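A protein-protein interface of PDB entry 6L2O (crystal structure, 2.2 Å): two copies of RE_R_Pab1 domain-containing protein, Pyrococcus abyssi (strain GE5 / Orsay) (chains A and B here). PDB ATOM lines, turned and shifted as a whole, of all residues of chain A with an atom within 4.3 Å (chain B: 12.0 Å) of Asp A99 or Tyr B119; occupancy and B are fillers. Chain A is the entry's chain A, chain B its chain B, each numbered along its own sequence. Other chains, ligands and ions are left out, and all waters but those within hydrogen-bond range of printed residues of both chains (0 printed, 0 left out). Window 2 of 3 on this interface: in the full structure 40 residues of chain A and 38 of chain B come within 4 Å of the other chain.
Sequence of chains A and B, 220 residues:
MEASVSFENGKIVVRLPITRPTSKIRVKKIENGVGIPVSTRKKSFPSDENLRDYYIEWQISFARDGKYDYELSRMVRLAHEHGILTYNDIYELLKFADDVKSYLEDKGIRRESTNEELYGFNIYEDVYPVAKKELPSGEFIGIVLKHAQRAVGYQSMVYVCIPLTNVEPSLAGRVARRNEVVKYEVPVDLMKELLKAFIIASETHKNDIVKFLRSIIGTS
Printed residues of chain A that touch a printed residue of chain B: Phe A96, Asp A99, Val A100, Lys A101, Ser A102 and Ile A200. Printed residues of chain B that touch a printed residue of chain A: Leu B118, Tyr B119 and Phe B121. Hydrophobic or aromatic side chains of chain B that line the printed part of chain A: Leu B118, Tyr B119 and Phe B121. Among the printed residues, 9 pairs touch across the chains.
No position is printed for both chains. Of the 9 pairs that touch across the chains among the printed residues, none has its exchanged pair printed and touching as well.
Of chain B, only Tyr B119 (3.8 Å) comes within 4 Å of Asp A99. Tyr B119 touches six residues of chain A. Phe A96 touches just one residue of chain B: Tyr B119. Val A100 touches just one residue of chain B: Tyr B119. Lys A101 touches one residue of chain B. Printed residues of chain B within 4 Å of Ser A102: Leu B118 and Tyr B119. Of chain B, only Leu B118 (3.3 Å), Tyr B119 (3.8 Å) and Phe B121 (3.5 Å) come within 4 Å of Ile A200. Printed residues of chain A within 4 Å of Phe B121: Ile A200 (3.5 Å). Printed residues of chain A within 4 Å of Leu B118: Ser A102 and Ile A200. The nearest residue of chain B that does not touch Asp A99 is Leu B118 (9.3 Å). The nearest printed residue of chain A that does not touch Phe B121 is Phe A96 (6.1 Å).
Phe A96 touches Tyr B119 (CZ to CB, 3.7 Å). O of Asp A99 touches OH of Tyr B119 (3.8 Å). OH of Tyr B119 touches CA of Val A100 (3.6 Å). Leu B118 touches Ser A102. Ser A102 touches Tyr B119. Leu B118 touches Ile A200. CG2 of Ile A200 touches CD2 of Tyr B119 (3.8 Å). Phe B121 touches Ile A200 (CD1 to CD1, 3.5 Å).
N of Lys A101 is in hydrogen-bond range of OH of Tyr B119 (3.3 Å).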
ATOM      1  N   LYS A  95     -12.923  13.054 -30.154  1.00  0.00           N
ATOM      2  CA  LYS A  95     -12.753  13.567 -28.800  1.00  0.00           C
ATOM      3  C   LYS A  95     -13.872  14.527 -28.430  1.00  0.00           C
ATOM      4  O   LYS A  95     -14.200  14.658 -27.249  1.00  0.00           O
ATOM      5  CB  LYS A  95     -11.390  14.236 -28.665  1.00  0.00           C
ATOM      6  CG  LYS A  95     -10.244  13.250 -28.482  1.00  0.00           C
ATOM      7  CD  LYS A  95     -10.471  12.387 -27.245  1.00  0.00           C
ATOM      8  CE  LYS A  95      -9.688  11.082 -27.315  1.00  0.00           C
ATOM      9  NZ  LYS A  95     -10.265  10.124 -28.304  1.00  0.00           N
ATOM     10  N   PHE A  96     -14.464  15.207 -29.418  1.00  0.00           N
ATOM     11  CA  PHE A  96     -15.662  15.998 -29.148  1.00  0.00           C
ATOM     12  C   PHE A  96     -16.851  15.093 -28.862  1.00  0.00           C
ATOM     13  O   PHE A  96     -17.643  15.366 -27.951  1.00  0.00           O
ATOM     14  CB  PHE A  96     -15.956  16.922 -30.330  1.00  0.00           C
ATOM     15  CG  PHE A  96     -17.295  17.612 -30.261  1.00  0.00           C
ATOM     16  CD1 PHE A  96     -17.476  18.728 -29.463  1.00  0.00           C
ATOM     17  CD2 PHE A  96     -18.365  17.156 -31.012  1.00  0.00           C
ATOM     18  CE1 PHE A  96     -18.705  19.369 -29.405  1.00  0.00           C
ATOM     19  CE2 PHE A  96     -19.598  17.791 -30.956  1.00  0.00           C
ATOM     20  CZ  PHE A  96     -19.766  18.899 -30.156  1.00  0.00           C
ATOM     21  N   ALA A  97     -16.984  14.002 -29.622  1.00  0.00           N
ATOM     22  CA  ALA A  97     -18.082  13.070 -29.395  1.00  0.00           C
ATOM     23  C   ALA A  97     -17.944  12.358 -28.058  1.00  0.00           C
ATOM     24  O   ALA A  97     -18.953  12.068 -27.407  1.00  0.00           O
ATOM     25  CB  ALA A  97     -18.156  12.051 -30.532  1.00  0.00           C
ATOM     26  N   ASP A  98     -16.712  12.076 -27.630  1.00  0.00           N
ATOM     27  CA  ASP A  98     -16.508  11.416 -26.348  1.00  0.00           C
ATOM     28  C   ASP A  98     -16.884  12.322 -25.181  1.00  0.00           C
ATOM     29  O   ASP A  98     -17.274  11.830 -24.117  1.00  0.00           O
ATOM     30  CB  ASP A  98     -15.054  10.959 -26.225  1.00  0.00           C
ATOM     31  CG  ASP A  98     -14.797  10.172 -24.957  1.00  0.00           C
ATOM     32  OD1 ASP A  98     -15.367   9.069 -24.816  1.00  0.00           O
ATOM     33  OD2 ASP A  98     -14.027  10.656 -24.101  1.00  0.00           O
ATOM     34  N   ASP A  99     -16.777  13.639 -25.361  1.00  0.00           N
ATOM     35  CA  ASP A  99     -17.123  14.590 -24.316  1.00  0.00           C
ATOM     36  C   ASP A  99     -18.599  14.969 -24.315  1.00  0.00           C
ATOM     37  O   ASP A  99     -19.115  15.397 -23.275  1.00  0.00           O
ATOM     38  CB  ASP A  99     -16.269  15.856 -24.453  1.00  0.00           C
ATOM     39  CG  ASP A  99     -14.790  15.586 -24.238  1.00  0.00           C
ATOM     40  OD1 ASP A  99     -13.956  16.347 -24.778  1.00  0.00           O
ATOM     41  OD2 ASP A  99     -14.460  14.610 -23.532  1.00  0.00           O
ATOM     42  N   VAL A 100     -19.289  14.822 -25.447  1.00  0.00           N
ATOM     43  CA  VAL A 100     -20.706  15.152 -25.514  1.00  0.00           C
ATOM     44  C   VAL A 100     -21.508  14.087 -24.777  1.00  0.00           C
ATOM     45  O   VAL A 100     -21.391  12.889 -25.067  1.00  0.00           O
ATOM     46  CB  VAL A 100     -21.158  15.281 -26.978  1.00  0.00           C
ATOM     47  CG1 VAL A 100     -22.672  15.170 -27.087  1.00  0.00           C
ATOM     48  CG2 VAL A 100     -20.673  16.598 -27.576  1.00  0.00           C
ATOM     49  N   LYS A 101     -22.327  14.523 -23.811  1.00  0.00           N
ATOM     50  CA  LYS A 101     -23.176  13.616 -23.045  1.00  0.00           C
ATOM     51  C   LYS A 101     -24.632  14.054 -22.930  1.00  0.00           C
ATOM     52  O   LYS A 101     -25.452  13.262 -22.449  1.00  0.00           O
ATOM     53  CB  LYS A 101     -22.612  13.413 -21.630  1.00  0.00           C
ATOM     54  CG  LYS A 101     -21.160  12.981 -21.599  1.00  0.00           C
ATOM     55  CD  LYS A 101     -20.419  13.609 -20.431  1.00  0.00           C
ATOM     56  CE  LYS A 101     -18.934  13.281 -20.487  1.00  0.00           C
ATOM     57  NZ  LYS A 101     -18.139  14.165 -19.590  1.00  0.00           N
ATOM     58  N   SER A 102     -24.981  15.272 -23.338  1.00  0.00           N
ATOM     59  CA  SER A 102     -26.368  15.703 -23.444  1.00  0.00           C
ATOM     60  C   SER A 102     -26.693  15.961 -24.911  1.00  0.00           C
ATOM     61  O   SER A 102     -25.835  16.414 -25.676  1.00  0.00           O
ATOM     62  CB  SER A 102     -26.630  16.960 -22.610  1.00  0.00           C
ATOM     63  OG  SER A 102     -25.717  17.988 -22.947  1.00  0.00           O
ATOM     64  N   ILE A 200     -24.397  15.744 -31.548  1.00  0.00           N
ATOM     65  CA  ILE A 200     -25.211  16.281 -30.459  1.00  0.00           C
ATOM     66  C   ILE A 200     -26.704  16.065 -30.656  1.00  0.00           C
ATOM     67  O   ILE A 200     -27.483  16.336 -29.727  1.00  0.00           O
ATOM     68  CB  ILE A 200     -24.978  17.792 -30.251  1.00  0.00           C
ATOM     69  CG1 ILE A 200     -25.617  18.592 -31.386  1.00  0.00           C
ATOM     70  CG2 ILE A 200     -23.495  18.103 -30.115  1.00  0.00           C
ATOM     71  CD1 ILE A 200     -25.729  20.071 -31.095  1.00  0.00           C
ATOM     72  N   THR B 114     -34.359  30.684 -26.577  1.00  0.00           N
ATOM     73  CA  THR B 114     -34.013  30.285 -25.222  1.00  0.00           C
ATOM     74  C   THR B 114     -32.530  30.533 -24.992  1.00  0.00           C
ATOM     75  O   THR B 114     -31.736  30.576 -25.937  1.00  0.00           O
ATOM     76  CB  THR B 114     -34.350  28.811 -24.951  1.00  0.00           C
ATOM     77  OG1 THR B 114     -33.295  27.981 -25.448  1.00  0.00           O
ATOM     78  CG2 THR B 114     -35.659  28.419 -25.624  1.00  0.00           C
ATOM     79  N   ASN B 115     -32.161  30.688 -23.723  1.00  0.00           N
ATOM     80  CA  ASN B 115     -30.815  31.098 -23.354  1.00  0.00           C
ATOM     81  C   ASN B 115     -29.872  29.923 -23.126  1.00  0.00           C
ATOM     82  O   ASN B 115     -28.904  30.061 -22.369  1.00  0.00           O
ATOM     83  CB  ASN B 115     -30.865  31.976 -22.101  1.00  0.00           C
ATOM     84  CG  ASN B 115     -31.611  31.313 -20.955  1.00  0.00           C
ATOM     85  OD1 ASN B 115     -32.443  30.429 -21.169  1.00  0.00           O
ATOM     86  ND2 ASN B 115     -31.311  31.733 -19.729  1.00  0.00           N
ATOM     87  N   GLU B 116     -30.113  28.785 -23.768  1.00  0.00           N
ATOM     88  CA  GLU B 116     -29.278  27.610 -23.580  1.00  0.00           C
ATOM     89  C   GLU B 116     -28.540  27.271 -24.869  1.00  0.00           C
ATOM     90  O   GLU B 116     -29.011  27.555 -25.974  1.00  0.00           O
ATOM     91  CB  GLU B 116     -30.112  26.412 -23.110  1.00  0.00           C
ATOM     92  CG  GLU B 116     -31.280  26.082 -24.008  1.00  0.00           C
ATOM     93  CD  GLU B 116     -32.432  25.417 -23.278  1.00  0.00           C
ATOM     94  OE1 GLU B 116     -33.536  25.347 -23.862  1.00  0.00           O
ATOM     95  OE2 GLU B 116     -32.237  24.965 -22.129  1.00  0.00           O
ATOM     96  N   GLU B 117     -27.366  26.663 -24.710  1.00  0.00           N
ATOM     97  CA  GLU B 117     -26.515  26.285 -25.827  1.00  0.00           C
ATOM     98  C   GLU B 117     -26.122  24.823 -25.697  1.00  0.00           C
ATOM     99  O   GLU B 117     -25.755  24.361 -24.613  1.00  0.00           O
ATOM    100  CB  GLU B 117     -25.260  27.158 -25.885  1.00  0.00           C
ATOM    101  CG  GLU B 117     -25.516  28.592 -26.310  1.00  0.00           C
ATOM    102  CD  GLU B 117     -24.307  29.220 -26.974  1.00  0.00           C
ATOM    103  OE1 GLU B 117     -23.333  28.484 -27.247  1.00  0.00           O
ATOM    104  OE2 GLU B 117     -24.329  30.446 -27.222  1.00  0.00           O
ATOM    105  N   LEU B 118     -26.200  24.096 -26.809  1.00  0.00           N
ATOM    106  CA  LEU B 118     -25.824  22.686 -26.858  1.00  0.00           C
ATOM    107  C   LEU B 118     -24.555  22.568 -27.697  1.00  0.00           C
ATOM    108  O   LEU B 118     -24.599  22.326 -28.905  1.00  0.00           O
ATOM    109  CB  LEU B 118     -26.956  21.840 -27.424  1.00  0.00           C
ATOM    110  CG  LEU B 118     -26.874  20.337 -27.145  1.00  0.00           C
ATOM    111  CD1 LEU B 118     -26.763  20.066 -25.646  1.00  0.00           C
ATOM    112  CD2 LEU B 118     -28.075  19.627 -27.729  1.00  0.00           C
ATOM    113  N   TYR B 119     -23.412  22.745 -27.039  1.00  0.00           N
ATOM    114  CA  TYR B 119     -22.099  22.617 -27.671  1.00  0.00           C
ATOM    115  C   TYR B 119     -22.010  23.496 -28.919  1.00  0.00           C
ATOM    116  O   TYR B 119     -21.791  23.027 -30.035  1.00  0.00           O
ATOM    117  CB  TYR B 119     -21.798  21.151 -27.996  1.00  0.00           C
ATOM    118  CG  TYR B 119     -21.889  20.241 -26.792  1.00  0.00           C
ATOM    119  CD1 TYR B 119     -20.857  20.181 -25.865  1.00  0.00           C
ATOM    120  CD2 TYR B 119     -23.013  19.451 -26.577  1.00  0.00           C
ATOM    121  CE1 TYR B 119     -20.936  19.356 -24.760  1.00  0.00           C
ATOM    122  CE2 TYR B 119     -23.100  18.622 -25.476  1.00  0.00           C
ATOM    123  CZ  TYR B 119     -22.057  18.578 -24.567  1.00  0.00           C
ATOM    124  OH  TYR B 119     -22.136  17.755 -23.465  1.00  0.00           O
ATOM    125  N   GLY B 120     -22.200  24.795 -28.705  1.00  0.00           N
ATOM    126  CA  GLY B 120     -22.115  25.771 -29.768  1.00  0.00           C
ATOM    127  C   GLY B 120     -23.363  25.926 -30.610  1.00  0.00           C
ATOM    128  O   GLY B 120     -23.337  26.686 -31.587  1.00  0.00           O
ATOM    129  N   PHE B 121     -24.449  25.241 -30.271  1.00  0.00           N
ATOM    130  CA  PHE B 121     -25.700  25.331 -31.015  1.00  0.00           C
ATOM    131  C   PHE B 121     -26.731  26.048 -30.153  1.00  0.00           C
ATOM    132  O   PHE B 121     -26.989  25.637 -29.016  1.00  0.00           O
ATOM    133  CB  PHE B 121     -26.200  23.942 -31.419  1.00  0.00           C
ATOM    134  CG  PHE B 121     -25.479  23.351 -32.611  1.00  0.00           C
ATOM    135  CD1 PHE B 121     -24.180  22.878 -32.494  1.00  0.00           C
ATOM    136  CD2 PHE B 121     -26.107  23.261 -33.843  1.00  0.00           C
ATOM    137  CE1 PHE B 121     -23.519  22.326 -33.586  1.00  0.00           C
ATOM    138  CE2 PHE B 121     -25.451  22.710 -34.941  1.00  0.00           C
ATOM    139  CZ  PHE B 121     -24.157  22.243 -34.810  1.00  0.00           C
ATOM    140  N   ASN B 122     -27.303  27.128 -30.682  1.00  0.00           N
ATOM    141  CA  ASN B 122     -28.384  27.809 -29.983  1.00  0.00           C
ATOM    142  C   ASN B 122     -29.633  26.941 -30.019  1.00  0.00           C
ATOM    143  O   ASN B 122     -29.997  26.399 -31.068  1.00  0.00           O
ATOM    144  CB  ASN B 122     -28.666  29.170 -30.620  1.00  0.00           C
ATOM    145  CG  ASN B 122     -27.509  30.138 -30.470  1.00  0.00           C
ATOM    146  OD1 ASN B 122     -26.703  30.026 -29.548  1.00  0.00           O
ATOM    147  ND2 ASN B 122     -27.422  31.098 -31.386  1.00  0.00           N
ATOM    148  N   ILE B 123     -30.277  26.799 -28.870  1.00  0.00           N
ATOM    149  CA  ILE B 123     -31.479  25.986 -28.723  1.00  0.00           C
ATOM    150  C   ILE B 123     -32.693  26.895 -28.806  1.00  0.00           C
ATOM    151  O   ILE B 123     -32.712  27.983 -28.217  1.00  0.00           O
ATOM    152  CB  ILE B 123     -31.454  25.216 -27.386  1.00  0.00           C
ATOM    153  CG1 ILE B 123     -30.200  24.343 -27.292  1.00  0.00           C
ATOM    154  CG2 ILE B 123     -32.728  24.403 -27.195  1.00  0.00           C
ATOM    155  CD1 ILE B 123     -30.208  23.179 -28.256  1.00  0.00           C
ATOM    156  N   TYR B 124     -33.714  26.456 -29.532  1.00  0.00           N
ATOM    157  CA  TYR B 124     -34.973  27.176 -29.602  1.00  0.00           C
ATOM    158  C   TYR B 124     -36.107  26.218 -29.268  1.00  0.00           C
ATOM    159  O   TYR B 124     -35.899  25.017 -29.073  1.00  0.00           O
ATOM    160  CB  TYR B 124     -35.178  27.816 -30.985  1.00  0.00           C
ATOM    161  CG  TYR B 124     -34.104  28.824 -31.350  1.00  0.00           C
ATOM    162  CD1 TYR B 124     -34.341  30.188 -31.248  1.00  0.00           C
ATOM    163  CD2 TYR B 124     -32.854  28.409 -31.792  1.00  0.00           C
ATOM    164  CE1 TYR B 124     -33.359  31.113 -31.576  1.00  0.00           C
ATOM    165  CE2 TYR B 124     -31.869  29.325 -32.119  1.00  0.00           C
ATOM    166  CZ  TYR B 124     -32.129  30.675 -32.013  1.00  0.00           C
ATOM    167  OH  TYR B 124     -31.155  31.590 -32.341  1.00  0.00           O
